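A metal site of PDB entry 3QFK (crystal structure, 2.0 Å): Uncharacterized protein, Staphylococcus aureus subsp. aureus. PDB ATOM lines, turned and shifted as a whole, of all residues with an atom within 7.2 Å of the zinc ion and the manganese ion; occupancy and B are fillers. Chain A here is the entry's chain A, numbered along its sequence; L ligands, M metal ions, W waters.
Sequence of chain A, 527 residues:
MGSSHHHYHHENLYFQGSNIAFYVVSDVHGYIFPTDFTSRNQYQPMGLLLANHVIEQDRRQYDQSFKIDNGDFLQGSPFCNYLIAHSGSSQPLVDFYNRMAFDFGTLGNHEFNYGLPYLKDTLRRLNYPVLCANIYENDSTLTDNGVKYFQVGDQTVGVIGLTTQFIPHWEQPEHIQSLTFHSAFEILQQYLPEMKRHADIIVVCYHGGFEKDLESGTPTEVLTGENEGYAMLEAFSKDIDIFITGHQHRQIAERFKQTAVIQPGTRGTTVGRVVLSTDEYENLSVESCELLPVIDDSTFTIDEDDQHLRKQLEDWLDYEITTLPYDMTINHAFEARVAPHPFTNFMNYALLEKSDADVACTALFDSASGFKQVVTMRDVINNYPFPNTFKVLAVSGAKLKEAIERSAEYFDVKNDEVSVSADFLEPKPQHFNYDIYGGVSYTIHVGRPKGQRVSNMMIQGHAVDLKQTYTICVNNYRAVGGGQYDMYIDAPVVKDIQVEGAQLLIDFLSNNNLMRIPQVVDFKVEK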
ATOM      1  N   SER A  26     -20.639 -19.866 -36.173  1.00  0.00           N
ATOM      2  CA  SER A  26     -21.000 -19.190 -34.948  1.00  0.00           C
ATOM      3  C   SER A  26     -22.099 -19.941 -34.255  1.00  0.00           C
ATOM      4  O   SER A  26     -22.872 -20.658 -34.877  1.00  0.00           O
ATOM      5  CB  SER A  26     -21.477 -17.765 -35.243  1.00  0.00           C
ATOM      6  OG  SER A  26     -21.728 -17.062 -34.033  1.00  0.00           O
ATOM      7  N   ASP A  27     -22.152 -19.788 -32.950  1.00  0.00           N
ATOM      8  CA  ASP A  27     -23.182 -20.399 -32.155  1.00  0.00           C
ATOM      9  C   ASP A  27     -23.396 -21.887 -32.448  1.00  0.00           C
ATOM     10  O   ASP A  27     -24.531 -22.354 -32.603  1.00  0.00           O
ATOM     11  CB  ASP A  27     -24.485 -19.615 -32.319  1.00  0.00           C
ATOM     12  CG  ASP A  27     -24.362 -18.183 -31.861  1.00  0.00           C
ATOM     13  OD1 ASP A  27     -24.703 -17.927 -30.702  1.00  0.00           O
ATOM     14  OD2 ASP A  27     -23.918 -17.317 -32.646  1.00  0.00           O
ATOM     15  N   VAL A  28     -22.293 -22.615 -32.556  1.00  0.00           N
ATOM     16  CA  VAL A  28     -22.313 -24.035 -32.778  1.00  0.00           C
ATOM     17  C   VAL A  28     -22.971 -24.757 -31.616  1.00  0.00           C
ATOM     18  O   VAL A  28     -23.665 -25.763 -31.800  1.00  0.00           O
ATOM     19  CB  VAL A  28     -20.907 -24.573 -33.057  1.00  0.00           C
ATOM     20  CG1 VAL A  28     -20.935 -26.085 -33.177  1.00  0.00           C
ATOM     21  CG2 VAL A  28     -20.387 -23.903 -34.319  1.00  0.00           C
ATOM     22  N   HIS A  29     -22.748 -24.220 -30.421  1.00  0.00           N
ATOM     23  CA  HIS A  29     -23.402 -24.696 -29.212  1.00  0.00           C
ATOM     24  C   HIS A  29     -23.197 -26.184 -28.849  1.00  0.00           C
ATOM     25  O   HIS A  29     -24.064 -26.806 -28.252  1.00  0.00           O
ATOM     26  CB  HIS A  29     -24.917 -24.360 -29.258  1.00  0.00           C
ATOM     27  CG  HIS A  29     -25.240 -22.937 -28.877  1.00  0.00           C
ATOM     28  ND1 HIS A  29     -25.061 -22.471 -27.587  1.00  0.00           N
ATOM     29  CD2 HIS A  29     -25.731 -21.896 -29.592  1.00  0.00           C
ATOM     30  CE1 HIS A  29     -25.417 -21.196 -27.532  1.00  0.00           C
ATOM     31  NE2 HIS A  29     -25.823 -20.824 -28.744  1.00  0.00           N
ATOM     32  N   ASN A  70     -17.149 -17.959 -33.947  1.00  0.00           N
ATOM     33  CA  ASN A  70     -17.581 -16.690 -33.343  1.00  0.00           C
ATOM     34  C   ASN A  70     -18.366 -16.753 -32.026  1.00  0.00           C
ATOM     35  O   ASN A  70     -19.244 -15.912 -31.776  1.00  0.00           O
ATOM     36  CB  ASN A  70     -18.321 -15.873 -34.407  1.00  0.00           C
ATOM     37  CG  ASN A  70     -18.493 -14.406 -34.009  1.00  0.00           C
ATOM     38  OD1 ASN A  70     -17.599 -13.779 -33.417  1.00  0.00           O
ATOM     39  ND2 ASN A  70     -19.664 -13.845 -34.345  1.00  0.00           N
ATOM     40  N   GLY A  71     -18.050 -17.724 -31.164  1.00  0.00           N
ATOM     41  CA  GLY A  71     -18.667 -17.784 -29.837  1.00  0.00           C
ATOM     42  C   GLY A  71     -19.863 -18.697 -29.630  1.00  0.00           C
ATOM     43  O   GLY A  71     -20.486 -19.142 -30.590  1.00  0.00           O
ATOM     44  N   ASP A  72     -20.200 -18.916 -28.361  1.00  0.00           N
ATOM     45  CA  ASP A  72     -21.270 -19.839 -27.983  1.00  0.00           C
ATOM     46  C   ASP A  72     -20.945 -21.248 -28.487  1.00  0.00           C
ATOM     47  O   ASP A  72     -21.765 -21.880 -29.147  1.00  0.00           O
ATOM     48  CB  ASP A  72     -22.642 -19.335 -28.436  1.00  0.00           C
ATOM     49  CG  ASP A  72     -23.249 -18.377 -27.449  1.00  0.00           C
ATOM     50  OD1 ASP A  72     -22.559 -17.995 -26.493  1.00  0.00           O
ATOM     51  OD2 ASP A  72     -24.424 -18.042 -27.581  1.00  0.00           O
ATOM     52  N   PHE A  73     -19.739 -21.711 -28.149  1.00  0.00           N
ATOM     53  CA  PHE A  73     -19.261 -23.030 -28.563  1.00  0.00           C
ATOM     54  C   PHE A  73     -19.167 -24.034 -27.405  1.00  0.00           C
ATOM     55  O   PHE A  73     -19.086 -25.241 -27.629  1.00  0.00           O
ATOM     56  CB  PHE A  73     -17.856 -22.894 -29.216  1.00  0.00           C
ATOM     57  CG  PHE A  73     -16.761 -22.453 -28.267  1.00  0.00           C
ATOM     58  CD1 PHE A  73     -16.079 -23.372 -27.480  1.00  0.00           C
ATOM     59  CD2 PHE A  73     -16.435 -21.111 -28.150  1.00  0.00           C
ATOM     60  CE1 PHE A  73     -15.059 -22.961 -26.602  1.00  0.00           C
ATOM     61  CE2 PHE A  73     -15.416 -20.688 -27.281  1.00  0.00           C
ATOM     62  CZ  PHE A  73     -14.750 -21.621 -26.488  1.00  0.00           C
ATOM     63  N   GLN A  75     -21.385 -24.517 -24.632  1.00  0.00           N
ATOM     64  CA  GLN A  75     -22.624 -24.949 -24.016  1.00  0.00           C
ATOM     65  C   GLN A  75     -23.779 -24.952 -25.014  1.00  0.00           C
ATOM     66  O   GLN A  75     -23.787 -24.190 -25.967  1.00  0.00           O
ATOM     67  CB  GLN A  75     -22.967 -23.974 -22.863  1.00  0.00           C
ATOM     68  CG  GLN A  75     -24.287 -24.252 -22.095  1.00  0.00           C
ATOM     69  CD  GLN A  75     -25.556 -23.755 -22.798  1.00  0.00           C
ATOM     70  OE1 GLN A  75     -25.498 -22.900 -23.666  1.00  0.00           O
ATOM     71  NE2 GLN A  75     -26.692 -24.281 -22.394  1.00  0.00           N
ATOM     72  N   LEU A 107     -15.419 -15.034 -27.738  1.00  0.00           N
ATOM     73  CA  LEU A 107     -16.194 -15.520 -26.632  1.00  0.00           C
ATOM     74  C   LEU A 107     -17.632 -15.126 -26.781  1.00  0.00           C
ATOM     75  O   LEU A 107     -17.943 -13.949 -27.025  1.00  0.00           O
ATOM     76  CB  LEU A 107     -15.702 -14.917 -25.312  1.00  0.00           C
ATOM     77  CG  LEU A 107     -14.320 -15.330 -24.796  1.00  0.00           C
ATOM     78  CD1 LEU A 107     -13.977 -14.484 -23.560  1.00  0.00           C
ATOM     79  CD2 LEU A 107     -14.327 -16.802 -24.486  1.00  0.00           C
ATOM     80  N   GLY A 108     -18.519 -16.095 -26.601  1.00  0.00           N
ATOM     81  CA  GLY A 108     -19.960 -15.812 -26.580  1.00  0.00           C
ATOM     82  C   GLY A 108     -20.425 -15.761 -25.122  1.00  0.00           C
ATOM     83  O   GLY A 108     -19.659 -16.103 -24.228  1.00  0.00           O
ATOM     84  N   ASN A 109     -21.662 -15.293 -24.862  1.00  0.00           N
ATOM     85  CA  ASN A 109     -22.163 -15.252 -23.487  1.00  0.00           C
ATOM     86  C   ASN A 109     -22.216 -16.639 -22.812  1.00  0.00           C
ATOM     87  O   ASN A 109     -21.994 -16.754 -21.604  1.00  0.00           O
ATOM     88  CB  ASN A 109     -23.552 -14.588 -23.370  1.00  0.00           C
ATOM     89  CG  ASN A 109     -24.567 -15.179 -24.335  1.00  0.00           C
ATOM     90  OD1 ASN A 109     -24.343 -15.187 -25.559  1.00  0.00           O
ATOM     91  ND2 ASN A 109     -25.696 -15.656 -23.806  1.00  0.00           N
ATOM     92  N   HIS A 110     -22.501 -17.677 -23.588  1.00  0.00           N
ATOM     93  CA  HIS A 110     -22.592 -19.016 -23.024  1.00  0.00           C
ATOM     94  C   HIS A 110     -21.265 -19.640 -22.565  1.00  0.00           C
ATOM     95  O   HIS A 110     -21.300 -20.609 -21.804  1.00  0.00           O
ATOM     96  CB  HIS A 110     -23.428 -19.957 -23.897  1.00  0.00           C
ATOM     97  CG  HIS A 110     -24.880 -19.587 -23.923  1.00  0.00           C
ATOM     98  ND1 HIS A 110     -25.736 -19.874 -22.879  1.00  0.00           N
ATOM     99  CD2 HIS A 110     -25.615 -18.909 -24.842  1.00  0.00           C
ATOM    100  CE1 HIS A 110     -26.943 -19.412 -23.160  1.00  0.00           C
ATOM    101  NE2 HIS A 110     -26.901 -18.810 -24.340  1.00  0.00           N
ATOM    102  N   THR A 164     -20.827  -9.353 -26.587  1.00  0.00           N
ATOM    103  CA  THR A 164     -21.964  -8.601 -26.020  1.00  0.00           C
ATOM    104  C   THR A 164     -21.685  -8.234 -24.547  1.00  0.00           C
ATOM    105  O   THR A 164     -21.271  -9.089 -23.734  1.00  0.00           O
ATOM    106  CB  THR A 164     -23.339  -9.351 -26.178  1.00  0.00           C
ATOM    107  OG1 THR A 164     -24.382  -8.624 -25.495  1.00  0.00           O
ATOM    108  CG2 THR A 164     -23.264 -10.800 -25.615  1.00  0.00           C
ATOM    109  N   TRP A 170     -27.495 -11.862 -17.334  1.00  0.00           N
ATOM    110  CA  TRP A 170     -27.830 -13.252 -17.562  1.00  0.00           C
ATOM    111  C   TRP A 170     -27.157 -14.293 -16.677  1.00  0.00           C
ATOM    112  O   TRP A 170     -27.765 -15.294 -16.303  1.00  0.00           O
ATOM    113  CB  TRP A 170     -27.454 -13.615 -19.020  1.00  0.00           C
ATOM    114  CG  TRP A 170     -28.097 -12.706 -20.059  1.00  0.00           C
ATOM    115  CD1 TRP A 170     -29.374 -12.194 -20.032  1.00  0.00           C
ATOM    116  CD2 TRP A 170     -27.551 -12.340 -21.328  1.00  0.00           C
ATOM    117  NE1 TRP A 170     -29.614 -11.451 -21.167  1.00  0.00           N
ATOM    118  CE2 TRP A 170     -28.518 -11.535 -21.985  1.00  0.00           C
ATOM    119  CE3 TRP A 170     -26.319 -12.573 -21.960  1.00  0.00           C
ATOM    120  CZ2 TRP A 170     -28.298 -10.998 -23.248  1.00  0.00           C
ATOM    121  CZ3 TRP A 170     -26.094 -12.012 -23.202  1.00  0.00           C
ATOM    122  CH2 TRP A 170     -27.079 -11.230 -23.831  1.00  0.00           C
ATOM    123  N   HIS A 207     -19.443 -11.142 -31.080  1.00  0.00           N
ATOM    124  CA  HIS A 207     -20.445 -12.060 -30.649  1.00  0.00           C
ATOM    125  C   HIS A 207     -21.618 -11.224 -30.111  1.00  0.00           C
ATOM    126  O   HIS A 207     -21.782 -11.029 -28.898  1.00  0.00           O
ATOM    127  CB  HIS A 207     -20.016 -13.030 -29.577  1.00  0.00           C
ATOM    128  CG  HIS A 207     -21.050 -14.061 -29.333  1.00  0.00           C
ATOM    129  ND1 HIS A 207     -21.169 -15.186 -30.126  1.00  0.00           N
ATOM    130  CD2 HIS A 207     -22.130 -14.069 -28.510  1.00  0.00           C
ATOM    131  CE1 HIS A 207     -22.229 -15.879 -29.736  1.00  0.00           C
ATOM    132  NE2 HIS A 207     -22.832 -15.220 -28.759  1.00  0.00           N
ATOM    133  N   GLY A 208     -22.347 -10.657 -31.060  1.00  0.00           N
ATOM    134  CA  GLY A 208     -23.518  -9.841 -30.785  1.00  0.00           C
ATOM    135  C   GLY A 208     -24.128  -9.606 -32.148  1.00  0.00           C
ATOM    136  O   GLY A 208     -23.518  -9.933 -33.189  1.00  0.00           O
ATOM    137  N   GLU A 226     -27.549  -4.592 -25.445  1.00  0.00           N
ATOM    138  CA  GLU A 226     -27.232  -5.998 -25.614  1.00  0.00           C
ATOM    139  C   GLU A 226     -26.599  -6.176 -26.976  1.00  0.00           C
ATOM    140  O   GLU A 226     -25.589  -6.831 -27.113  1.00  0.00           O
ATOM    141  CB  GLU A 226     -28.467  -6.885 -25.500  1.00  0.00           C
ATOM    142  CG  GLU A 226     -28.178  -8.379 -25.821  1.00  0.00           C
ATOM    143  CD  GLU A 226     -29.427  -9.243 -25.842  1.00  0.00           C
ATOM    144  OE1 GLU A 226     -29.315 -10.412 -26.252  1.00  0.00           O
ATOM    145  OE2 GLU A 226     -30.514  -8.736 -25.464  1.00  0.00           O
ATOM    146  N   GLY A 246     -22.883 -12.716 -34.563  1.00  0.00           N
ATOM    147  CA  GLY A 246     -23.487 -13.959 -34.076  1.00  0.00           C
ATOM    148  C   GLY A 246     -24.525 -13.592 -33.037  1.00  0.00           C
ATOM    149  O   GLY A 246     -25.157 -12.551 -33.154  1.00  0.00           O
ATOM    150  N   HIS A 247     -24.685 -14.455 -32.046  1.00  0.00           N
ATOM    151  CA  HIS A 247     -25.571 -14.240 -30.896  1.00  0.00           C
ATOM    152  C   HIS A 247     -27.087 -14.335 -31.154  1.00  0.00           C
ATOM    153  O   HIS A 247     -27.790 -14.957 -30.375  1.00  0.00           O
ATOM    154  CB  HIS A 247     -25.243 -12.886 -30.220  1.00  0.00           C
ATOM    155  CG  HIS A 247     -26.024 -12.645 -28.957  1.00  0.00           C
ATOM    156  ND1 HIS A 247     -25.905 -13.464 -27.860  1.00  0.00           N
ATOM    157  CD2 HIS A 247     -26.912 -11.671 -28.623  1.00  0.00           C
ATOM    158  CE1 HIS A 247     -26.695 -13.018 -26.901  1.00  0.00           C
ATOM    159  NE2 HIS A 247     -27.311 -11.927 -27.331  1.00  0.00           N
ATOM    160  N   GLN A 248     -27.558 -13.730 -32.228  1.00  0.00           N
ATOM    161  CA  GLN A 248     -28.976 -13.698 -32.543  1.00  0.00           C
ATOM    162  C   GLN A 248     -29.443 -14.903 -33.334  1.00  0.00           C
ATOM    163  O   GLN A 248     -30.635 -15.052 -33.546  1.00  0.00           O
ATOM    164  CB  GLN A 248     -29.307 -12.430 -33.303  1.00  0.00           C
ATOM    165  CG  GLN A 248     -29.255 -11.160 -32.456  1.00  0.00           C
ATOM    166  CD  GLN A 248     -29.546  -9.932 -33.306  1.00  0.00           C
ATOM    167  OE1 GLN A 248     -29.035  -9.808 -34.425  1.00  0.00           O
ATOM    168  NE2 GLN A 248     -30.381  -9.046 -32.797  1.00  0.00           N
ATOM    169  N   HIS A 249     -28.514 -15.747 -33.791  1.00  0.00           N
ATOM    170  CA  HIS A 249     -28.859 -16.964 -34.520  1.00  0.00           C
ATOM    171  C   HIS A 249     -29.554 -16.689 -35.850  1.00  0.00           C
ATOM    172  O   HIS A 249     -30.304 -17.533 -36.347  1.00  0.00           O
ATOM    173  CB  HIS A 249     -29.771 -17.845 -33.643  1.00  0.00           C
ATOM    174  CG  HIS A 249     -29.119 -18.343 -32.396  1.00  0.00           C
ATOM    175  ND1 HIS A 249     -29.675 -19.337 -31.614  1.00  0.00           N
ATOM    176  CD2 HIS A 249     -27.910 -18.071 -31.843  1.00  0.00           C
ATOM    177  CE1 HIS A 249     -28.873 -19.589 -30.588  1.00  0.00           C
ATOM    178  NE2 HIS A 249     -27.790 -18.840 -30.715  1.00  0.00           N
ATOM    179  N   GLY A 265     -26.045 -18.064 -38.632  1.00  0.00           N
ATOM    180  CA  GLY A 265     -26.994 -18.947 -37.968  1.00  0.00           C
ATOM    181  C   GLY A 265     -26.507 -19.589 -36.707  1.00  0.00           C
ATOM    182  O   GLY A 265     -25.800 -18.967 -35.890  1.00  0.00           O
ATOM    183  N   THR A 266     -26.859 -20.863 -36.555  1.00  0.00           N
ATOM    184  CA  THR A 266     -26.516 -21.626 -35.381  1.00  0.00           C
ATOM    185  C   THR A 266     -26.506 -23.130 -35.669  1.00  0.00           C
ATOM    186  O   THR A 266     -27.097 -23.578 -36.646  1.00  0.00           O
ATOM    187  CB  THR A 266     -27.543 -21.319 -34.232  1.00  0.00           C
ATOM    188  OG1 THR A 266     -27.160 -21.981 -33.006  1.00  0.00           O
ATOM    189  CG2 THR A 266     -28.985 -21.740 -34.645  1.00  0.00           C
ATOM    190  N   LYS A 428     -35.268 -13.260 -33.270  1.00  0.00           N
ATOM    191  CA  LYS A 428     -34.923 -14.575 -32.704  1.00  0.00           C
ATOM    192  C   LYS A 428     -36.054 -15.038 -31.767  1.00  0.00           C
ATOM    193  O   LYS A 428     -36.499 -14.272 -30.937  1.00  0.00           O
ATOM    194  CB  LYS A 428     -33.605 -14.531 -31.916  1.00  0.00           C
ATOM    195  CG  LYS A 428     -33.263 -15.868 -31.262  1.00  0.00           C
ATOM    196  CD  LYS A 428     -31.993 -15.826 -30.416  1.00  0.00           C
ATOM    197  CE  LYS A 428     -31.768 -17.164 -29.722  1.00  0.00           C
ATOM    198  NZ  LYS A 428     -30.635 -17.145 -28.749  1.00  0.00           N
HETATM  199  C1  LIG L   1     -30.589 -18.284 -24.236  1.00  0.00           C
HETATM  200  O1  LIG L   1     -31.195 -19.063 -25.007  1.00  0.00           O
HETATM  201  O2  LIG L   1     -29.760 -17.470 -24.680  1.00  0.00           O
HETATM  202  C2  LIG L   1     -30.831 -18.321 -22.787  1.00  0.00           C
HETATM  203  O3  LIG L   1     -30.012 -17.797 -22.058  1.00  0.00           O
HETATM  204  C3  LIG L   1     -32.058 -19.008 -22.206  1.00  0.00           C
HETATM  205  C4  LIG L   1     -32.561 -18.337 -20.921  1.00  0.00           C
HETATM  206  C5  LIG L   1     -32.630 -19.310 -19.762  1.00  0.00           C
HETATM  207  O4  LIG L   1     -33.721 -19.544 -19.218  1.00  0.00           O
HETATM  208  O5  LIG L   1     -31.572 -19.854 -19.386  1.00  0.00           O
HETATM  209 ZN    ZN M   1     -26.054 -18.580 -29.100  1.00  0.00          ZN
HETATM  210 MN    MN M   2     -24.875 -15.679 -27.580  1.00  0.00          MN
HETATM  211  O   HOH W   1     -26.989 -16.466 -28.609  1.00  0.00           O
HETATM  212  O   HOH W   2     -27.834 -16.513 -26.074  1.00  0.00           O
HETATM  213  O   HOH W   3     -27.739 -18.725 -27.372  1.00  0.00           O
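An oxygen (O2) of the ligand lies within hydrogen-bond range of a ring nitrogen (NE2) of His 110 (3.2 Å).
ND2 of Asn 109 sits close to NE2 of His 110 (3.4 Å).
The backbone carbonyl oxygen (O) of Asp 27 lies within hydrogen-bond range of the side-chain hydroxyl (OG1) of Thr 266.
The backbone carbonyl oxygen of Gly 71 is in hydrogen-bond range of the backbone NH of Asp 27 (3.0 Å).
The backbone carbonyl oxygen (O) of Gln 75 lies within hydrogen-bond range of a ring nitrogen (ND1) of His 29.
The side-chain carboxylate (OD1) of Asp 72 sits at hydrogen-bond distance from the backbone NH (N) of His 110, at 2.9 Å.
O of His 207 is in hydrogen-bond range of N of Thr 164 (3.0 Å).
O of Asn 70 is in hydrogen-bond range of ND1 of His 207, at 2.6 Å.
A ring nitrogen (NE2) of His 247 lies within hydrogen-bond range of the side-chain carboxylate (OE1) of Glu 226, at 2.7 Å.
Within 4 Å of the zinc ion: Asp 27, His 29, Asp 72 and His 249.
The nearest printed residue that does not touch the manganese ion is His 110 (4.3 Å).
The zinc ion is bound by the side-chain carboxylate (OD1) of Asp 27, a ring nitrogen (NE2) of His 29, the side-chain carboxylate (OD2) of Asp 72, water W1, a ring nitrogen (NE2) of His 249 and water W3.
The manganese ion is bound by OD1 of Asn 109, 2.1 Å away.
A ring nitrogen (NE2) of His 207 binds the manganese ion (2.4 Å).
The side-chain carboxylate (OD2) of Asp 72 is bound to the manganese ion, 2.4 Å away.
ND1 of His 247 is bound to the manganese ion (2.5 Å).
Water W1 binds the manganese ion.
Water W2 lies within hydrogen-bond range of an oxygen (O2) of the ligand (2.6 Å), a ring nitrogen (NE2) of His 110 (3.0 Å) and the side-chain amide nitrogen (ND2) of Asn 109 (3.2 Å).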
